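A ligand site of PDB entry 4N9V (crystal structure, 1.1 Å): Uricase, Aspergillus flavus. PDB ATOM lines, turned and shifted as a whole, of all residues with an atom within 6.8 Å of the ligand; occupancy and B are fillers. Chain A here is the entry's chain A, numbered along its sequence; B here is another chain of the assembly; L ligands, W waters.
N3 of the ligand lies within hydrogen-bond range of N of Thr 58 of chain B (2.8 Å).
An oxygen (O2) of the ligand is in hydrogen-bond range of the side-chain amide nitrogen (NE2) of Gln 229.
A nitrogen (N2) of the ligand sits close to the side-chain amide nitrogen (ND2) of Asn 255.
N3 of the ligand is in hydrogen-bond range of OG1 of Thr 58 of chain B (3.2 Å).
The guanidinium group (NH2) of Arg 177 lies within hydrogen-bond range of an oxygen (O1) of the ligand.
N of Val 228 lies within hydrogen-bond range of O1 of the ligand, 2.9 Å away.
Residues that only touch the ligand: Phe 160 (3.3 Å), Ser 227 (3.5 Å), Ile 55 of chain B (3.5 Å), Ala 57 of chain B (3.6 Å), Leu 171 (3.7 Å), Tyr 9 of chain B (3.8 Å) and Asp 59 of chain B (3.8 Å).
Along chain A the residues within 4 Å of the ligand span positions 160 to 255.
The nearest printed residue that does not touch the ligand is Ile 289 (4.001 Å).
N of Asn 255 sits at hydrogen-bond distance from O of Gly 287 (2.8 Å).
The backbone NH (N) of Gln 229 lies close to the side-chain hydroxyl (OG) of Ser 227 (3.3 Å).
A ring nitrogen (NE2) of His 257 sits at hydrogen-bond distance from the backbone carbonyl oxygen (O) of Asn 255, 3.3 Å away.
OG1 of Thr 58 of chain B lies within hydrogen-bond range of NZ of Lys 11 of chain B, 2.8 Å away.
N of Arg 177 sits at hydrogen-bond distance from O of Ser 158 (2.9 Å).
The backbone carbonyl oxygen (O) of Ser 227 is in hydrogen-bond range of the side-chain hydroxyl (OG) of Ser 225 (2.9 Å).
The side-chain hydroxyl (OH) of Tyr 9 of chain B is in hydrogen-bond range of the backbone carbonyl oxygen (O) of Val 56 of chain B (2.6 Å).
Water W1 lies within hydrogen-bond range of a nitrogen (N5) of the ligand (2.9 Å) and the guanidinium group (NH1) of Arg 177 (3.4 Å).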
ATOM      1  N   SER A 158      10.184 -32.222   1.962  1.00  0.00           N
ATOM      2  CA  SER A 158      10.821 -30.945   1.805  1.00  0.00           C
ATOM      3  C   SER A 158      10.022 -30.217   0.722  1.00  0.00           C
ATOM      4  O   SER A 158       9.643 -30.827  -0.288  1.00  0.00           O
ATOM      5  CB  SER A 158      12.283 -31.116   1.399  1.00  0.00           C
ATOM      6  OG  SER A 158      12.869 -29.886   1.054  1.00  0.00           O
ATOM      7  N   GLN A 159       9.767 -28.944   0.956  1.00  0.00           N
ATOM      8  CA  GLN A 159       8.978 -28.100   0.071  1.00  0.00           C
ATOM      9  C   GLN A 159       9.697 -26.781  -0.135  1.00  0.00           C
ATOM     10  O   GLN A 159      10.524 -26.373   0.691  1.00  0.00           O
ATOM     11  CB  GLN A 159       7.595 -27.823   0.697  1.00  0.00           C
ATOM     12  CG  GLN A 159       6.914 -29.068   1.171  1.00  0.00           C
ATOM     13  CD  GLN A 159       5.494 -28.863   1.581  1.00  0.00           C
ATOM     14  OE1 GLN A 159       4.765 -28.073   0.997  1.00  0.00           O
ATOM     15  NE2 GLN A 159       5.078 -29.583   2.603  1.00  0.00           N
ATOM     16  N   PHE A 160       9.370 -26.085  -1.207  1.00  0.00           N
ATOM     17  CA  PHE A 160       9.820 -24.716  -1.371  1.00  0.00           C
ATOM     18  C   PHE A 160       8.903 -24.004  -2.347  1.00  0.00           C
ATOM     19  O   PHE A 160       8.991 -24.151  -3.568  1.00  0.00           O
ATOM     20  CB  PHE A 160      11.283 -24.633  -1.803  1.00  0.00           C
ATOM     21  CG  PHE A 160      11.835 -23.237  -1.715  1.00  0.00           C
ATOM     22  CD1 PHE A 160      11.903 -22.596  -0.486  1.00  0.00           C
ATOM     23  CD2 PHE A 160      12.269 -22.562  -2.846  1.00  0.00           C
ATOM     24  CE1 PHE A 160      12.413 -21.313  -0.393  1.00  0.00           C
ATOM     25  CE2 PHE A 160      12.775 -21.293  -2.752  1.00  0.00           C
ATOM     26  CZ  PHE A 160      12.841 -20.644  -1.518  1.00  0.00           C
ATOM     27  N   PHE A 163       8.078 -18.175  -2.656  1.00  0.00           N
ATOM     28  CA  PHE A 163       9.192 -17.259  -2.773  1.00  0.00           C
ATOM     29  C   PHE A 163       8.926 -16.145  -3.781  1.00  0.00           C
ATOM     30  O   PHE A 163       8.001 -16.228  -4.594  1.00  0.00           O
ATOM     31  CB  PHE A 163      10.485 -18.027  -3.095  1.00  0.00           C
ATOM     32  CG  PHE A 163      10.372 -18.946  -4.278  1.00  0.00           C
ATOM     33  CD1 PHE A 163       9.992 -20.273  -4.095  1.00  0.00           C
ATOM     34  CD2 PHE A 163      10.627 -18.488  -5.559  1.00  0.00           C
ATOM     35  CE1 PHE A 163       9.878 -21.130  -5.187  1.00  0.00           C
ATOM     36  CE2 PHE A 163      10.530 -19.348  -6.641  1.00  0.00           C
ATOM     37  CZ  PHE A 163      10.151 -20.653  -6.452  1.00  0.00           C
ATOM     38  N   LEU A 171      12.595 -20.595 -11.246  1.00  0.00           N
ATOM     39  CA  LEU A 171      12.377 -21.753 -10.396  1.00  0.00           C
ATOM     40  C   LEU A 171      10.906 -22.040 -10.192  1.00  0.00           C
ATOM     41  O   LEU A 171      10.148 -21.158  -9.796  1.00  0.00           O
ATOM     42  CB  LEU A 171      13.043 -21.530  -9.034  1.00  0.00           C
ATOM     43  CG  LEU A 171      12.939 -22.658  -8.002  1.00  0.00           C
ATOM     44  CD1 LEU A 171      13.716 -23.906  -8.471  1.00  0.00           C
ATOM     45  CD2 LEU A 171      13.468 -22.211  -6.658  1.00  0.00           C
ATOM     46  N   ARG A 177      10.198 -32.191  -2.778  1.00  0.00           N
ATOM     47  CA  ARG A 177      11.536 -32.250  -3.359  1.00  0.00           C
ATOM     48  C   ARG A 177      12.467 -33.049  -2.449  1.00  0.00           C
ATOM     49  O   ARG A 177      12.150 -33.321  -1.284  1.00  0.00           O
ATOM     50  CB  ARG A 177      12.107 -30.850  -3.595  1.00  0.00           C
ATOM     51  CG  ARG A 177      12.350 -30.070  -2.322  1.00  0.00           C
ATOM     52  CD  ARG A 177      12.957 -28.693  -2.546  1.00  0.00           C
ATOM     53  NE  ARG A 177      13.272 -28.092  -1.257  1.00  0.00           N
ATOM     54  CZ  ARG A 177      13.961 -26.968  -1.097  1.00  0.00           C
ATOM     55  NH1 ARG A 177      14.304 -26.223  -2.130  1.00  0.00           N
ATOM     56  NH2 ARG A 177      14.280 -26.566   0.142  1.00  0.00           N
ATOM     57  N   LEU A 179      15.881 -32.981  -0.228  1.00  0.00           N
ATOM     58  CA  LEU A 179      16.741 -32.045   0.491  1.00  0.00           C
ATOM     59  C   LEU A 179      17.959 -32.803   0.996  1.00  0.00           C
ATOM     60  O   LEU A 179      17.822 -33.788   1.734  1.00  0.00           O
ATOM     61  CB  LEU A 179      15.985 -31.409   1.647  1.00  0.00           C
ATOM     62  CG  LEU A 179      16.812 -30.494   2.546  1.00  0.00           C
ATOM     63  CD1 LEU A 179      17.400 -29.341   1.771  1.00  0.00           C
ATOM     64  CD2 LEU A 179      15.960 -29.988   3.692  1.00  0.00           C
ATOM     65  N   SER A 225       9.652 -29.716   5.691  1.00  0.00           N
ATOM     66  CA  SER A 225      10.392 -28.483   5.655  1.00  0.00           C
ATOM     67  C   SER A 225       9.834 -27.476   4.673  1.00  0.00           C
ATOM     68  O   SER A 225       9.589 -27.790   3.516  1.00  0.00           O
ATOM     69  CB  SER A 225      11.836 -28.824   5.273  1.00  0.00           C
ATOM     70  OG  SER A 225      12.580 -27.673   5.015  1.00  0.00           O
ATOM     71  N   ALA A 226       9.623 -26.255   5.145  1.00  0.00           N
ATOM     72  CA  ALA A 226       9.187 -25.150   4.285  1.00  0.00           C
ATOM     73  C   ALA A 226      10.304 -24.498   3.484  1.00  0.00           C
ATOM     74  O   ALA A 226      10.067 -23.799   2.497  1.00  0.00           O
ATOM     75  CB  ALA A 226       8.483 -24.102   5.130  1.00  0.00           C
ATOM     76  N   SER A 227      11.522 -24.708   3.968  1.00  0.00           N
ATOM     77  CA  SER A 227      12.743 -24.138   3.400  1.00  0.00           C
ATOM     78  C   SER A 227      13.897 -24.608   4.276  1.00  0.00           C
ATOM     79  O   SER A 227      13.687 -25.003   5.427  1.00  0.00           O
ATOM     80  CB  SER A 227      12.768 -22.604   3.394  1.00  0.00           C
ATOM     81  OG  SER A 227      12.758 -22.122   4.717  1.00  0.00           O
ATOM     82  N   VAL A 228      15.115 -24.495   3.777  1.00  0.00           N
ATOM     83  CA  VAL A 228      16.267 -24.746   4.622  1.00  0.00           C
ATOM     84  C   VAL A 228      16.276 -23.772   5.793  1.00  0.00           C
ATOM     85  O   VAL A 228      16.546 -24.150   6.941  1.00  0.00           O
ATOM     86  CB  VAL A 228      17.574 -24.668   3.811  1.00  0.00           C
ATOM     87  CG1 VAL A 228      18.787 -24.845   4.716  1.00  0.00           C
ATOM     88  CG2 VAL A 228      17.573 -25.744   2.719  1.00  0.00           C
ATOM     89  N   GLN A 229      15.960 -22.513   5.497  1.00  0.00           N
ATOM     90  CA  GLN A 229      15.907 -21.463   6.516  1.00  0.00           C
ATOM     91  C   GLN A 229      15.011 -21.871   7.696  1.00  0.00           C
ATOM     92  O   GLN A 229      15.393 -21.730   8.869  1.00  0.00           O
ATOM     93  CB  GLN A 229      15.333 -20.181   5.888  1.00  0.00           C
ATOM     94  CG  GLN A 229      16.261 -19.422   4.913  1.00  0.00           C
ATOM     95  CD  GLN A 229      16.243 -19.895   3.458  1.00  0.00           C
ATOM     96  OE1 GLN A 229      15.890 -21.052   3.149  1.00  0.00           O
ATOM     97  NE2 GLN A 229      16.631 -19.009   2.563  1.00  0.00           N
ATOM     98  N   ASN A 255      22.548 -26.238   0.156  1.00  0.00           N
ATOM     99  CA  ASN A 255      21.421 -26.968  -0.421  1.00  0.00           C
ATOM    100  C   ASN A 255      22.000 -27.686  -1.635  1.00  0.00           C
ATOM    101  O   ASN A 255      22.290 -27.065  -2.651  1.00  0.00           O
ATOM    102  CB  ASN A 255      20.298 -26.011  -0.802  1.00  0.00           C
ATOM    103  CG  ASN A 255      18.972 -26.705  -1.054  1.00  0.00           C
ATOM    104  OD1 ASN A 255      18.871 -27.941  -1.006  1.00  0.00           O
ATOM    105  ND2 ASN A 255      17.952 -25.923  -1.320  1.00  0.00           N
ATOM    106  N   HIS A 257      21.680 -29.690  -4.519  1.00  0.00           N
ATOM    107  CA  HIS A 257      20.486 -29.886  -5.323  1.00  0.00           C
ATOM    108  C   HIS A 257      20.494 -31.219  -6.070  1.00  0.00           C
ATOM    109  O   HIS A 257      21.522 -31.664  -6.568  1.00  0.00           O
ATOM    110  CB  HIS A 257      20.347 -28.754  -6.345  1.00  0.00           C
ATOM    111  CG  HIS A 257      20.391 -27.381  -5.745  1.00  0.00           C
ATOM    112  ND1 HIS A 257      19.420 -26.900  -4.879  1.00  0.00           N
ATOM    113  CD2 HIS A 257      21.288 -26.374  -5.879  1.00  0.00           C
ATOM    114  CE1 HIS A 257      19.739 -25.666  -4.515  1.00  0.00           C
ATOM    115  NE2 HIS A 257      20.860 -25.319  -5.102  1.00  0.00           N
ATOM    116  N   GLY A 287      22.906 -23.834  -3.194  1.00  0.00           N
ATOM    117  CA  GLY A 287      22.453 -22.831  -2.241  1.00  0.00           C
ATOM    118  C   GLY A 287      23.333 -22.887  -1.006  1.00  0.00           C
ATOM    119  O   GLY A 287      23.883 -23.926  -0.670  1.00  0.00           O
ATOM    120  N   ILE A 289      22.905 -21.414   2.950  1.00  0.00           N
ATOM    121  CA  ILE A 289      21.941 -20.794   3.851  1.00  0.00           C
ATOM    122  C   ILE A 289      22.584 -20.725   5.230  1.00  0.00           C
ATOM    123  O   ILE A 289      23.068 -21.748   5.734  1.00  0.00           O
ATOM    124  CB  ILE A 289      20.621 -21.608   3.904  1.00  0.00           C
ATOM    125  CG1 ILE A 289      20.174 -22.093   2.503  1.00  0.00           C
ATOM    126  CG2 ILE A 289      19.541 -20.827   4.633  1.00  0.00           C
ATOM    127  CD1 ILE A 289      19.878 -21.031   1.468  1.00  0.00           C
ATOM    128  N   TYR B   9      22.041 -15.618   3.002  1.00  0.00           N
ATOM    129  CA  TYR B   9      21.775 -16.796   2.195  1.00  0.00           C
ATOM    130  C   TYR B   9      21.993 -16.431   0.745  1.00  0.00           C
ATOM    131  O   TYR B   9      21.927 -15.261   0.367  1.00  0.00           O
ATOM    132  CB  TYR B   9      20.342 -17.318   2.447  1.00  0.00           C
ATOM    133  CG  TYR B   9      19.386 -16.532   1.602  1.00  0.00           C
ATOM    134  CD1 TYR B   9      19.047 -15.213   1.899  1.00  0.00           C
ATOM    135  CD2 TYR B   9      18.919 -17.054   0.410  1.00  0.00           C
ATOM    136  CE1 TYR B   9      18.269 -14.458   1.058  1.00  0.00           C
ATOM    137  CE2 TYR B   9      18.161 -16.320  -0.448  1.00  0.00           C
ATOM    138  CZ  TYR B   9      17.842 -15.020  -0.133  1.00  0.00           C
ATOM    139  OH  TYR B   9      17.086 -14.263  -0.969  1.00  0.00           O
ATOM    140  N   GLY B  10      22.241 -17.428  -0.095  1.00  0.00           N
ATOM    141  CA  GLY B  10      22.433 -17.148  -1.501  1.00  0.00           C
ATOM    142  C   GLY B  10      22.910 -18.375  -2.243  1.00  0.00           C
ATOM    143  O   GLY B  10      22.610 -19.495  -1.861  1.00  0.00           O
ATOM    144  N   LYS B  11      23.621 -18.135  -3.339  1.00  0.00           N
ATOM    145  CA  LYS B  11      24.098 -19.242  -4.167  1.00  0.00           C
ATOM    146  C   LYS B  11      25.621 -19.201  -4.189  1.00  0.00           C
ATOM    147  O   LYS B  11      26.212 -18.155  -4.388  1.00  0.00           O
ATOM    148  CB  LYS B  11      23.548 -19.176  -5.599  1.00  0.00           C
ATOM    149  CG  LYS B  11      23.758 -20.474  -6.374  1.00  0.00           C
ATOM    150  CD  LYS B  11      22.839 -21.608  -5.917  1.00  0.00           C
ATOM    151  CE  LYS B  11      21.610 -21.741  -6.810  1.00  0.00           C
ATOM    152  NZ  LYS B  11      20.582 -22.568  -6.154  1.00  0.00           N
ATOM    153  N   ASN B  52       8.385 -17.354   2.936  1.00  0.00           N
ATOM    154  CA  ASN B  52       9.260 -17.341   1.783  1.00  0.00           C
ATOM    155  C   ASN B  52       9.119 -16.108   0.901  1.00  0.00           C
ATOM    156  O   ASN B  52       9.899 -15.944  -0.020  1.00  0.00           O
ATOM    157  CB  ASN B  52       9.128 -18.627   0.967  1.00  0.00           C
ATOM    158  CG  ASN B  52       9.699 -19.808   1.718  1.00  0.00           C
ATOM    159  OD1 ASN B  52      10.623 -19.646   2.505  1.00  0.00           O
ATOM    160  ND2 ASN B  52       9.158 -20.995   1.471  1.00  0.00           N
ATOM    161  N   ILE B  55      12.204 -14.175   0.302  1.00  0.00           N
ATOM    162  CA  ILE B  55      13.327 -14.860  -0.316  1.00  0.00           C
ATOM    163  C   ILE B  55      13.380 -14.623  -1.822  1.00  0.00           C
ATOM    164  O   ILE B  55      12.466 -15.026  -2.560  1.00  0.00           O
ATOM    165  CB  ILE B  55      13.230 -16.381  -0.084  1.00  0.00           C
ATOM    166  CG1 ILE B  55      13.365 -16.719   1.406  1.00  0.00           C
ATOM    167  CG2 ILE B  55      14.307 -17.106  -0.878  1.00  0.00           C
ATOM    168  CD1 ILE B  55      13.294 -18.193   1.705  1.00  0.00           C
ATOM    169  N   VAL B  56      14.441 -13.970  -2.264  1.00  0.00           N
ATOM    170  CA  VAL B  56      14.862 -13.982  -3.646  1.00  0.00           C
ATOM    171  C   VAL B  56      15.535 -15.351  -3.797  1.00  0.00           C
ATOM    172  O   VAL B  56      16.564 -15.610  -3.186  1.00  0.00           O
ATOM    173  CB  VAL B  56      15.840 -12.835  -3.937  1.00  0.00           C
ATOM    174  CG1 VAL B  56      16.370 -12.927  -5.358  1.00  0.00           C
ATOM    175  CG2 VAL B  56      15.166 -11.476  -3.682  1.00  0.00           C
ATOM    176  N   ALA B  57      14.941 -16.247  -4.579  1.00  0.00           N
ATOM    177  CA  ALA B  57      15.401 -17.629  -4.593  1.00  0.00           C
ATOM    178  C   ALA B  57      16.868 -17.684  -4.968  1.00  0.00           C
ATOM    179  O   ALA B  57      17.340 -16.934  -5.814  1.00  0.00           O
ATOM    180  CB  ALA B  57      14.592 -18.456  -5.559  1.00  0.00           C
ATOM    181  N   THR B  58      17.600 -18.612  -4.362  1.00  0.00           N
ATOM    182  CA  THR B  58      18.995 -18.750  -4.716  1.00  0.00           C
ATOM    183  C   THR B  58      19.144 -19.113  -6.196  1.00  0.00           C
ATOM    184  O   THR B  58      20.094 -18.688  -6.835  1.00  0.00           O
ATOM    185  CB  THR B  58      19.735 -19.785  -3.823  1.00  0.00           C
ATOM    186  OG1 THR B  58      19.295 -21.103  -4.147  1.00  0.00           O
ATOM    187  CG2 THR B  58      19.496 -19.494  -2.345  1.00  0.00           C
ATOM    188  N   ASP B  59      18.178 -19.838  -6.736  1.00  0.00           N
ATOM    189  CA  ASP B  59      18.166 -20.143  -8.163  1.00  0.00           C
ATOM    190  C   ASP B  59      18.090 -18.851  -8.979  1.00  0.00           C
ATOM    191  O   ASP B  59      18.699 -18.744 -10.028  1.00  0.00           O
ATOM    192  CB  ASP B  59      16.984 -21.046  -8.507  1.00  0.00           C
ATOM    193  CG  ASP B  59      17.054 -21.540  -9.917  1.00  0.00           C
ATOM    194  OD1 ASP B  59      17.805 -22.515 -10.142  1.00  0.00           O
ATOM    195  OD2 ASP B  59      16.388 -20.954 -10.795  1.00  0.00           O
ATOM    196  N   SER B  60      17.304 -17.885  -8.499  1.00  0.00           N
ATOM    197  CA  SER B  60      17.182 -16.596  -9.163  1.00  0.00           C
ATOM    198  C   SER B  60      18.457 -15.784  -9.031  1.00  0.00           C
ATOM    199  O   SER B  60      18.834 -15.042  -9.938  1.00  0.00           O
ATOM    200  CB  SER B  60      16.008 -15.812  -8.601  1.00  0.00           C
ATOM    201  OG  SER B  60      14.837 -16.569  -8.703  1.00  0.00           O
HETATM  202  N1  LIG L   1      15.861 -21.938   0.317  1.00  0.00           N
HETATM  203  C1  LIG L   1      15.513 -23.242   0.008  1.00  0.00           C
HETATM  204  O1  LIG L   1      15.239 -24.010   0.937  1.00  0.00           O
HETATM  205  N2  LIG L   1      15.476 -23.660  -1.299  1.00  0.00           N
HETATM  206  C2  LIG L   1      15.751 -22.689  -2.236  1.00  0.00           C
HETATM  207  C3  LIG L   1      16.062 -21.383  -1.944  1.00  0.00           C
HETATM  208  C4  LIG L   1      16.142 -20.960  -0.609  1.00  0.00           C
HETATM  209  O2  LIG L   1      16.453 -19.825  -0.212  1.00  0.00           O
HETATM  210  N3  LIG L   1      16.248 -20.771  -3.114  1.00  0.00           N
HETATM  211  N4  LIG L   1      16.076 -21.613  -4.050  1.00  0.00           N
HETATM  212  N5  LIG L   1      15.800 -22.757  -3.569  1.00  0.00           N
HETATM  213  O   HOH W   1      15.690 -25.237  -5.023  1.00  0.00           O
